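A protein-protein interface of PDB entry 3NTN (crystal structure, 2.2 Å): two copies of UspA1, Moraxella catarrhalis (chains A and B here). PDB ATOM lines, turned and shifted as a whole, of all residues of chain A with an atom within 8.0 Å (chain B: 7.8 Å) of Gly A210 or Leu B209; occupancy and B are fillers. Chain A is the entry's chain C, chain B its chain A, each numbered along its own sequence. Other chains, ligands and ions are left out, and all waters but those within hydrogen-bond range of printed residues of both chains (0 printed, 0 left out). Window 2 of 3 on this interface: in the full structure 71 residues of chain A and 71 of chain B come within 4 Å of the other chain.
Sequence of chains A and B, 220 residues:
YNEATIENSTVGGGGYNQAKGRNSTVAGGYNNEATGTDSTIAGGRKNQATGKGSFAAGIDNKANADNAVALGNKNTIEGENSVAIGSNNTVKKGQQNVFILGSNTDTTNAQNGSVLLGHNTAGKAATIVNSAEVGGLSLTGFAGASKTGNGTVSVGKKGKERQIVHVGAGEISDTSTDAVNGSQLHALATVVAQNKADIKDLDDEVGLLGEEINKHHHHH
The backbone carbonyl oxygen (O) of Gly A210 is in hydrogen-bond range of the side-chain amide nitrogen (ND2) of Asn A214.
Leu B202 touches Asp A203 (CD1 to OD1, 3.8 Å).
Glu B205 touches Val A206 (CD to CG1, 3.9 Å).
CG2 of Val A206 touches CG2 of Val B206 (3.6 Å).
Leu B209 touches Val A206.
Gly A210 touches Leu B209 (N to CD1, 3.6 Å).
Leu B209 touches Ile A213 (O to CD1, 3.7 Å).
CD1 of Ile A213 touches CG1 of Ile B213, 3.4 Å away.
Asp A204 touches none of the printed residues of chain B.
Of the printed residues of chain B, Gly A210 touches Leu B209.
Printed residues of chain B within 4 Å of Ile A213: Leu B209 (3.7 Å) and Ile B213 (3.4 Å).
Lys A215 touches none of the printed residues of chain B.
Printed residues of chain A within 4 Å of Leu B202: Asp A203 (3.8 Å).
Of the printed residues of chain A, Glu B205 touches Val A206 (3.9 Å).
Of chain A, only Val A206, Gly A210 and Ile A213 come within 4 Å of Leu B209.
The nearest printed residue of chain B that does not touch Val A206 is Leu B202 (4.3 Å).
Of the 14 printed residues of chain B, 5 touch a printed residue of chain A.
Along chain B the printed residues that touch a printed residue of chain A span positions 202 to 213.
Of the 14 printed residues of chain A, 4 touch a printed residue of chain B.
Hydrophobic or aromatic side chains of chain A within 4 Å of the printed part of chain B: Val A206 and Ile A213.
Along chain A the printed residues that touch a printed residue of chain B span positions 203 to 213.
Among the printed residues, 7 pairs touch across the chains.
Val A206 touches Glu B205, but with the chains exchanged Glu A205 does not touch Val B206 (7.6 Å).
Val A206 touches its own counterpart, Val B206.
Val A206 touches Leu B209, but with the chains exchanged Leu A209 does not touch Val B206 (7.3 Å).
Gly A210 touches Leu B209, but with the chains exchanged Leu A209 does not touch Gly B210 (8.3 Å).
Positions printed for both chains: 203, 204, 205, 206, 207, 208, 209, 210, 211, 212, 213, 214 and 215.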
ATOM      1  N   ASP A 203       3.024  11.596 -13.658  1.00  0.00           N
ATOM      2  CA  ASP A 203       3.194  13.033 -13.381  1.00  0.00           C
ATOM      3  C   ASP A 203       4.206  13.299 -12.248  1.00  0.00           C
ATOM      4  O   ASP A 203       5.064  14.159 -12.382  1.00  0.00           O
ATOM      5  CB  ASP A 203       1.851  13.669 -13.025  1.00  0.00           C
ATOM      6  CG  ASP A 203       1.994  15.109 -12.655  1.00  0.00           C
ATOM      7  OD1 ASP A 203       2.237  15.958 -13.548  1.00  0.00           O
ATOM      8  OD2 ASP A 203       1.885  15.399 -11.450  1.00  0.00           O
ATOM      9  N   ASP A 204       4.072  12.556 -11.142  1.00  0.00           N
ATOM     10  CA  ASP A 204       5.063  12.577 -10.067  1.00  0.00           C
ATOM     11  C   ASP A 204       6.453  12.237 -10.607  1.00  0.00           C
ATOM     12  O   ASP A 204       7.439  12.946 -10.311  1.00  0.00           O
ATOM     13  CB  ASP A 204       4.678  11.600  -8.937  1.00  0.00           C
ATOM     14  CG  ASP A 204       3.477  12.108  -8.085  1.00  0.00           C
ATOM     15  OD1 ASP A 204       3.075  13.271  -8.296  1.00  0.00           O
ATOM     16  OD2 ASP A 204       2.938  11.347  -7.206  1.00  0.00           O
ATOM     17  N   GLU A 205       6.538  11.169 -11.397  1.00  0.00           N
ATOM     18  CA  GLU A 205       7.842  10.798 -11.945  1.00  0.00           C
ATOM     19  C   GLU A 205       8.453  11.897 -12.821  1.00  0.00           C
ATOM     20  O   GLU A 205       9.587  12.290 -12.614  1.00  0.00           O
ATOM     21  CB  GLU A 205       7.826   9.443 -12.654  1.00  0.00           C
ATOM     22  CG  GLU A 205       9.230   8.820 -12.701  1.00  0.00           C
ATOM     23  CD  GLU A 205       9.288   7.471 -13.411  1.00  0.00           C
ATOM     24  OE1 GLU A 205       8.198   6.887 -13.678  1.00  0.00           O
ATOM     25  OE2 GLU A 205      10.426   7.000 -13.703  1.00  0.00           O
ATOM     26  N   VAL A 206       7.698  12.396 -13.778  1.00  0.00           N
ATOM     27  CA  VAL A 206       8.142  13.561 -14.590  1.00  0.00           C
ATOM     28  C   VAL A 206       8.584  14.769 -13.744  1.00  0.00           C
ATOM     29  O   VAL A 206       9.619  15.343 -14.017  1.00  0.00           O
ATOM     30  CB  VAL A 206       7.055  13.969 -15.619  1.00  0.00           C
ATOM     31  CG1 VAL A 206       7.451  15.251 -16.395  1.00  0.00           C
ATOM     32  CG2 VAL A 206       6.809  12.816 -16.528  1.00  0.00           C
ATOM     33  N   GLY A 207       7.807  15.162 -12.740  1.00  0.00           N
ATOM     34  CA  GLY A 207       8.236  16.206 -11.791  1.00  0.00           C
ATOM     35  C   GLY A 207       9.626  15.967 -11.183  1.00  0.00           C
ATOM     36  O   GLY A 207      10.489  16.847 -11.216  1.00  0.00           O
ATOM     37  N   LEU A 208       9.833  14.777 -10.606  1.00  0.00           N
ATOM     38  CA  LEU A 208      11.118  14.405 -10.052  1.00  0.00           C
ATOM     39  C   LEU A 208      12.219  14.461 -11.118  1.00  0.00           C
ATOM     40  O   LEU A 208      13.293  14.966 -10.824  1.00  0.00           O
ATOM     41  CB  LEU A 208      11.103  12.997  -9.407  1.00  0.00           C
ATOM     42  CG  LEU A 208      10.347  12.721  -8.103  1.00  0.00           C
ATOM     43  CD1 LEU A 208      10.447  11.234  -7.680  1.00  0.00           C
ATOM     44  CD2 LEU A 208      10.803  13.649  -6.943  1.00  0.00           C
ATOM     45  N   LEU A 209      11.961  13.949 -12.332  1.00  0.00           N
ATOM     46  CA  LEU A 209      12.940  14.044 -13.394  1.00  0.00           C
ATOM     47  C   LEU A 209      13.278  15.503 -13.714  1.00  0.00           C
ATOM     48  O   LEU A 209      14.445  15.828 -13.948  1.00  0.00           O
ATOM     49  CB  LEU A 209      12.550  13.249 -14.657  1.00  0.00           C
ATOM     50  CG  LEU A 209      12.807  11.715 -14.662  1.00  0.00           C
ATOM     51  CD1 LEU A 209      12.616  11.078 -16.042  1.00  0.00           C
ATOM     52  CD2 LEU A 209      14.156  11.231 -14.086  1.00  0.00           C
ATOM     53  N   GLY A 210      12.280  16.388 -13.732  1.00  0.00           N
ATOM     54  CA  GLY A 210      12.553  17.813 -13.833  1.00  0.00           C
ATOM     55  C   GLY A 210      13.470  18.372 -12.745  1.00  0.00           C
ATOM     56  O   GLY A 210      14.293  19.228 -13.008  1.00  0.00           O
ATOM     57  N   GLU A 211      13.339  17.898 -11.518  1.00  0.00           N
ATOM     58  CA  GLU A 211      14.190  18.347 -10.445  1.00  0.00           C
ATOM     59  C   GLU A 211      15.613  17.928 -10.718  1.00  0.00           C
ATOM     60  O   GLU A 211      16.498  18.755 -10.539  1.00  0.00           O
ATOM     61  CB  GLU A 211      13.740  17.819  -9.081  1.00  0.00           C
ATOM     62  CG  GLU A 211      12.443  18.431  -8.526  1.00  0.00           C
ATOM     63  CD  GLU A 211      12.019  17.779  -7.188  1.00  0.00           C
ATOM     64  OE1 GLU A 211      12.839  17.011  -6.582  1.00  0.00           O
ATOM     65  OE2 GLU A 211      10.879  18.046  -6.724  1.00  0.00           O
ATOM     66  N   GLU A 212      15.833  16.680 -11.156  1.00  0.00           N
ATOM     67  CA  GLU A 212      17.182  16.190 -11.474  1.00  0.00           C
ATOM     68  C   GLU A 212      17.868  17.090 -12.503  1.00  0.00           C
ATOM     69  O   GLU A 212      18.992  17.565 -12.274  1.00  0.00           O
ATOM     70  CB  GLU A 212      17.190  14.723 -11.943  1.00  0.00           C
ATOM     71  CG  GLU A 212      16.973  13.699 -10.803  1.00  0.00           C
ATOM     72  CD  GLU A 212      18.169  13.582  -9.860  1.00  0.00           C
ATOM     73  OE1 GLU A 212      19.236  13.093 -10.287  1.00  0.00           O
ATOM     74  OE2 GLU A 212      18.034  13.968  -8.681  1.00  0.00           O
ATOM     75  N   ILE A 213      17.171  17.357 -13.612  1.00  0.00           N
ATOM     76  CA  ILE A 213      17.715  18.216 -14.651  1.00  0.00           C
ATOM     77  C   ILE A 213      18.118  19.584 -14.054  1.00  0.00           C
ATOM     78  O   ILE A 213      19.238  20.040 -14.245  1.00  0.00           O
ATOM     79  CB  ILE A 213      16.725  18.362 -15.821  1.00  0.00           C
ATOM     80  CG1 ILE A 213      16.632  17.038 -16.569  1.00  0.00           C
ATOM     81  CG2 ILE A 213      17.166  19.467 -16.791  1.00  0.00           C
ATOM     82  CD1 ILE A 213      15.596  17.028 -17.686  1.00  0.00           C
ATOM     83  N   ASN A 214      17.222  20.202 -13.298  1.00  0.00           N
ATOM     84  CA  ASN A 214      17.440  21.568 -12.790  1.00  0.00           C
ATOM     85  C   ASN A 214      18.600  21.608 -11.798  1.00  0.00           C
ATOM     86  O   ASN A 214      19.454  22.488 -11.868  1.00  0.00           O
ATOM     87  CB  ASN A 214      16.144  22.120 -12.169  1.00  0.00           C
ATOM     88  CG  ASN A 214      15.060  22.388 -13.215  1.00  0.00           C
ATOM     89  OD1 ASN A 214      15.350  22.589 -14.398  1.00  0.00           O
ATOM     90  ND2 ASN A 214      13.807  22.391 -12.777  1.00  0.00           N
ATOM     91  N   LYS A 215      18.625  20.627 -10.890  1.00  0.00           N
ATOM     92  CA  LYS A 215      19.737  20.433  -9.966  1.00  0.00           C
ATOM     93  C   LYS A 215      21.038  20.258 -10.757  1.00  0.00           C
ATOM     94  O   LYS A 215      21.951  21.057 -10.571  1.00  0.00           O
ATOM     95  CB  LYS A 215      19.453  19.246  -9.025  1.00  0.00           C
ATOM     96  CG  LYS A 215      20.658  18.534  -8.452  1.00  0.00           C
ATOM     97  CD  LYS A 215      20.275  17.138  -7.971  1.00  0.00           C
ATOM     98  CE  LYS A 215      21.499  16.340  -7.546  1.00  0.00           C
ATOM     99  NZ  LYS A 215      21.161  14.923  -7.249  1.00  0.00           N
ATOM    100  N   HIS A 216      21.122  19.280 -11.667  1.00  0.00           N
ATOM    101  CA  HIS A 216      22.388  19.071 -12.418  1.00  0.00           C
ATOM    102  C   HIS A 216      23.131  20.345 -12.873  1.00  0.00           C
ATOM    103  O   HIS A 216      24.321  20.457 -12.614  1.00  0.00           O
ATOM    104  CB  HIS A 216      22.266  18.101 -13.599  1.00  0.00           C
ATOM    105  CG  HIS A 216      23.557  17.915 -14.344  1.00  0.00           C
ATOM    106  ND1 HIS A 216      24.504  16.988 -13.968  1.00  0.00           N
ATOM    107  CD2 HIS A 216      24.078  18.568 -15.412  1.00  0.00           C
ATOM    108  CE1 HIS A 216      25.542  17.068 -14.782  1.00  0.00           C
ATOM    109  NE2 HIS A 216      25.310  18.015 -15.675  1.00  0.00           N
ATOM    110  N   LEU B 202       0.875  16.112 -20.005  1.00  0.00           N
ATOM    111  CA  LEU B 202       2.058  15.358 -19.599  1.00  0.00           C
ATOM    112  C   LEU B 202       3.053  15.100 -20.743  1.00  0.00           C
ATOM    113  O   LEU B 202       4.259  15.226 -20.568  1.00  0.00           O
ATOM    114  CB  LEU B 202       1.626  14.030 -18.998  1.00  0.00           C
ATOM    115  CG  LEU B 202       2.650  13.560 -18.023  1.00  0.00           C
ATOM    116  CD1 LEU B 202       2.970  14.675 -17.019  1.00  0.00           C
ATOM    117  CD2 LEU B 202       2.240  12.282 -17.371  1.00  0.00           C
ATOM    118  N   ASP B 203       2.541  14.694 -21.889  1.00  0.00           N
ATOM    119  CA  ASP B 203       3.338  14.471 -23.108  1.00  0.00           C
ATOM    120  C   ASP B 203       4.112  15.726 -23.508  1.00  0.00           C
ATOM    121  O   ASP B 203       5.301  15.647 -23.813  1.00  0.00           O
ATOM    122  CB  ASP B 203       2.425  14.039 -24.260  1.00  0.00           C
ATOM    123  CG  ASP B 203       3.170  13.890 -25.561  1.00  0.00           C
ATOM    124  OD1 ASP B 203       4.014  12.965 -25.704  1.00  0.00           O
ATOM    125  OD2 ASP B 203       2.898  14.725 -26.450  1.00  0.00           O
ATOM    126  N   ASP B 204       3.423  16.879 -23.516  1.00  0.00           N
ATOM    127  CA  ASP B 204       4.098  18.155 -23.769  1.00  0.00           C
ATOM    128  C   ASP B 204       5.238  18.319 -22.757  1.00  0.00           C
ATOM    129  O   ASP B 204       6.374  18.644 -23.158  1.00  0.00           O
ATOM    130  CB  ASP B 204       3.121  19.329 -23.705  1.00  0.00           C
ATOM    131  CG  ASP B 204       2.176  19.380 -24.924  1.00  0.00           C
ATOM    132  OD1 ASP B 204       2.439  18.675 -25.914  1.00  0.00           O
ATOM    133  OD2 ASP B 204       1.166  20.106 -24.898  1.00  0.00           O
ATOM    134  N   GLU B 205       4.949  18.075 -21.463  1.00  0.00           N
ATOM    135  CA  GLU B 205       5.978  18.250 -20.465  1.00  0.00           C
ATOM    136  C   GLU B 205       7.176  17.323 -20.705  1.00  0.00           C
ATOM    137  O   GLU B 205       8.312  17.781 -20.730  1.00  0.00           O
ATOM    138  CB  GLU B 205       5.442  18.162 -19.032  1.00  0.00           C
ATOM    139  CG  GLU B 205       6.348  18.921 -18.017  1.00  0.00           C
ATOM    140  CD  GLU B 205       5.903  18.783 -16.555  1.00  0.00           C
ATOM    141  OE1 GLU B 205       4.760  18.293 -16.307  1.00  0.00           O
ATOM    142  OE2 GLU B 205       6.698  19.175 -15.651  1.00  0.00           O
ATOM    143  N   VAL B 206       6.938  16.035 -20.889  1.00  0.00           N
ATOM    144  CA  VAL B 206       8.010  15.108 -21.244  1.00  0.00           C
ATOM    145  C   VAL B 206       8.847  15.548 -22.472  1.00  0.00           C
ATOM    146  O   VAL B 206      10.074  15.468 -22.431  1.00  0.00           O
ATOM    147  CB  VAL B 206       7.467  13.648 -21.424  1.00  0.00           C
ATOM    148  CG1 VAL B 206       8.547  12.707 -21.898  1.00  0.00           C
ATOM    149  CG2 VAL B 206       6.920  13.194 -20.155  1.00  0.00           C
ATOM    150  N   GLY B 207       8.203  16.002 -23.542  1.00  0.00           N
ATOM    151  CA  GLY B 207       8.915  16.541 -24.686  1.00  0.00           C
ATOM    152  C   GLY B 207       9.831  17.727 -24.349  1.00  0.00           C
ATOM    153  O   GLY B 207      10.999  17.768 -24.801  1.00  0.00           O
ATOM    154  N   LEU B 208       9.326  18.687 -23.566  1.00  0.00           N
ATOM    155  CA  LEU B 208      10.139  19.803 -23.139  1.00  0.00           C
ATOM    156  C   LEU B 208      11.315  19.311 -22.287  1.00  0.00           C
ATOM    157  O   LEU B 208      12.426  19.751 -22.490  1.00  0.00           O
ATOM    158  CB  LEU B 208       9.329  20.861 -22.366  1.00  0.00           C
ATOM    159  CG  LEU B 208       8.306  21.770 -23.071  1.00  0.00           C
ATOM    160  CD1 LEU B 208       7.621  22.712 -22.050  1.00  0.00           C
ATOM    161  CD2 LEU B 208       8.911  22.577 -24.224  1.00  0.00           C
ATOM    162  N   LEU B 209      11.064  18.400 -21.347  1.00  0.00           N
ATOM    163  CA  LEU B 209      12.139  17.841 -20.555  1.00  0.00           C
ATOM    164  C   LEU B 209      13.182  17.161 -21.442  1.00  0.00           C
ATOM    165  O   LEU B 209      14.376  17.345 -21.211  1.00  0.00           O
ATOM    166  CB  LEU B 209      11.640  16.899 -19.454  1.00  0.00           C
ATOM    167  CG  LEU B 209      11.104  17.531 -18.144  1.00  0.00           C
ATOM    168  CD1 LEU B 209      10.941  16.478 -17.095  1.00  0.00           C
ATOM    169  CD2 LEU B 209      11.899  18.702 -17.581  1.00  0.00           C
ATOM    170  N   GLY B 210      12.742  16.412 -22.457  1.00  0.00           N
ATOM    171  CA  GLY B 210      13.660  15.833 -23.442  1.00  0.00           C
ATOM    172  C   GLY B 210      14.555  16.859 -24.126  1.00  0.00           C
ATOM    173  O   GLY B 210      15.739  16.611 -24.307  1.00  0.00           O
ATOM    174  N   GLU B 211      14.001  18.024 -24.476  1.00  0.00           N
ATOM    175  CA  GLU B 211      14.744  19.040 -25.184  1.00  0.00           C
ATOM    176  C   GLU B 211      15.799  19.595 -24.285  1.00  0.00           C
ATOM    177  O   GLU B 211      16.918  19.801 -24.749  1.00  0.00           O
ATOM    178  CB  GLU B 211      13.859  20.167 -25.760  1.00  0.00           C
ATOM    179  CG  GLU B 211      12.766  19.657 -26.734  1.00  0.00           C
ATOM    180  CD  GLU B 211      12.059  20.759 -27.532  1.00  0.00           C
ATOM    181  OE1 GLU B 211      11.340  21.596 -26.932  1.00  0.00           O
ATOM    182  OE2 GLU B 211      12.218  20.768 -28.780  1.00  0.00           O
ATOM    183  N   GLU B 212      15.478  19.815 -23.008  1.00  0.00           N
ATOM    184  CA  GLU B 212      16.472  20.369 -22.085  1.00  0.00           C
ATOM    185  C   GLU B 212      17.678  19.477 -21.844  1.00  0.00           C
ATOM    186  O   GLU B 212      18.808  19.973 -21.763  1.00  0.00           O
ATOM    187  CB  GLU B 212      15.878  20.797 -20.759  1.00  0.00           C
ATOM    188  CG  GLU B 212      16.550  22.099 -20.289  1.00  0.00           C
ATOM    189  CD  GLU B 212      15.589  23.010 -19.566  1.00  0.00           C
ATOM    190  OE1 GLU B 212      14.426  22.560 -19.334  1.00  0.00           O
ATOM    191  OE2 GLU B 212      15.997  24.145 -19.227  1.00  0.00           O
ATOM    192  N   ILE B 213      17.448  18.169 -21.726  1.00  0.00           N
ATOM    193  CA  ILE B 213      18.546  17.234 -21.630  1.00  0.00           C
ATOM    194  C   ILE B 213      19.447  17.359 -22.858  1.00  0.00           C
ATOM    195  O   ILE B 213      20.655  17.557 -22.710  1.00  0.00           O
ATOM    196  CB  ILE B 213      18.054  15.789 -21.494  1.00  0.00           C
ATOM    197  CG1 ILE B 213      17.443  15.586 -20.123  1.00  0.00           C
ATOM    198  CG2 ILE B 213      19.195  14.799 -21.723  1.00  0.00           C
ATOM    199  CD1 ILE B 213      16.391  14.522 -20.129  1.00  0.00           C
ATOM    200  N   ASN B 214      18.852  17.276 -24.050  1.00  0.00           N
ATOM    201  CA  ASN B 214      19.602  17.360 -25.301  1.00  0.00           C
ATOM    202  C   ASN B 214      20.313  18.705 -25.461  1.00  0.00           C
ATOM    203  O   ASN B 214      21.457  18.761 -25.872  1.00  0.00           O
ATOM    204  CB  ASN B 214      18.701  17.026 -26.513  1.00  0.00           C
ATOM    205  CG  ASN B 214      18.261  15.543 -26.531  1.00  0.00           C
ATOM    206  OD1 ASN B 214      18.856  14.681 -25.862  1.00  0.00           O
ATOM    207  ND2 ASN B 214      17.216  15.253 -27.289  1.00  0.00           N
ATOM    208  N   LYS B 215      19.641  19.783 -25.093  1.00  0.00           N
ATOM    209  CA  LYS B 215      20.274  21.091 -25.003  1.00  0.00           C
ATOM    210  C   LYS B 215      21.500  21.036 -24.085  1.00  0.00           C
ATOM    211  O   LYS B 215      22.535  21.591 -24.430  1.00  0.00           O
ATOM    212  CB  LYS B 215      19.278  22.108 -24.457  1.00  0.00           C
ATOM    213  CG  LYS B 215      19.748  23.534 -24.468  1.00  0.00           C
ATOM    214  CD  LYS B 215      19.091  24.359 -23.352  1.00  0.00           C
ATOM    215  CE  LYS B 215      17.570  24.464 -23.495  1.00  0.00           C
ATOM    216  NZ  LYS B 215      17.143  25.314 -24.643  1.00  0.00           N
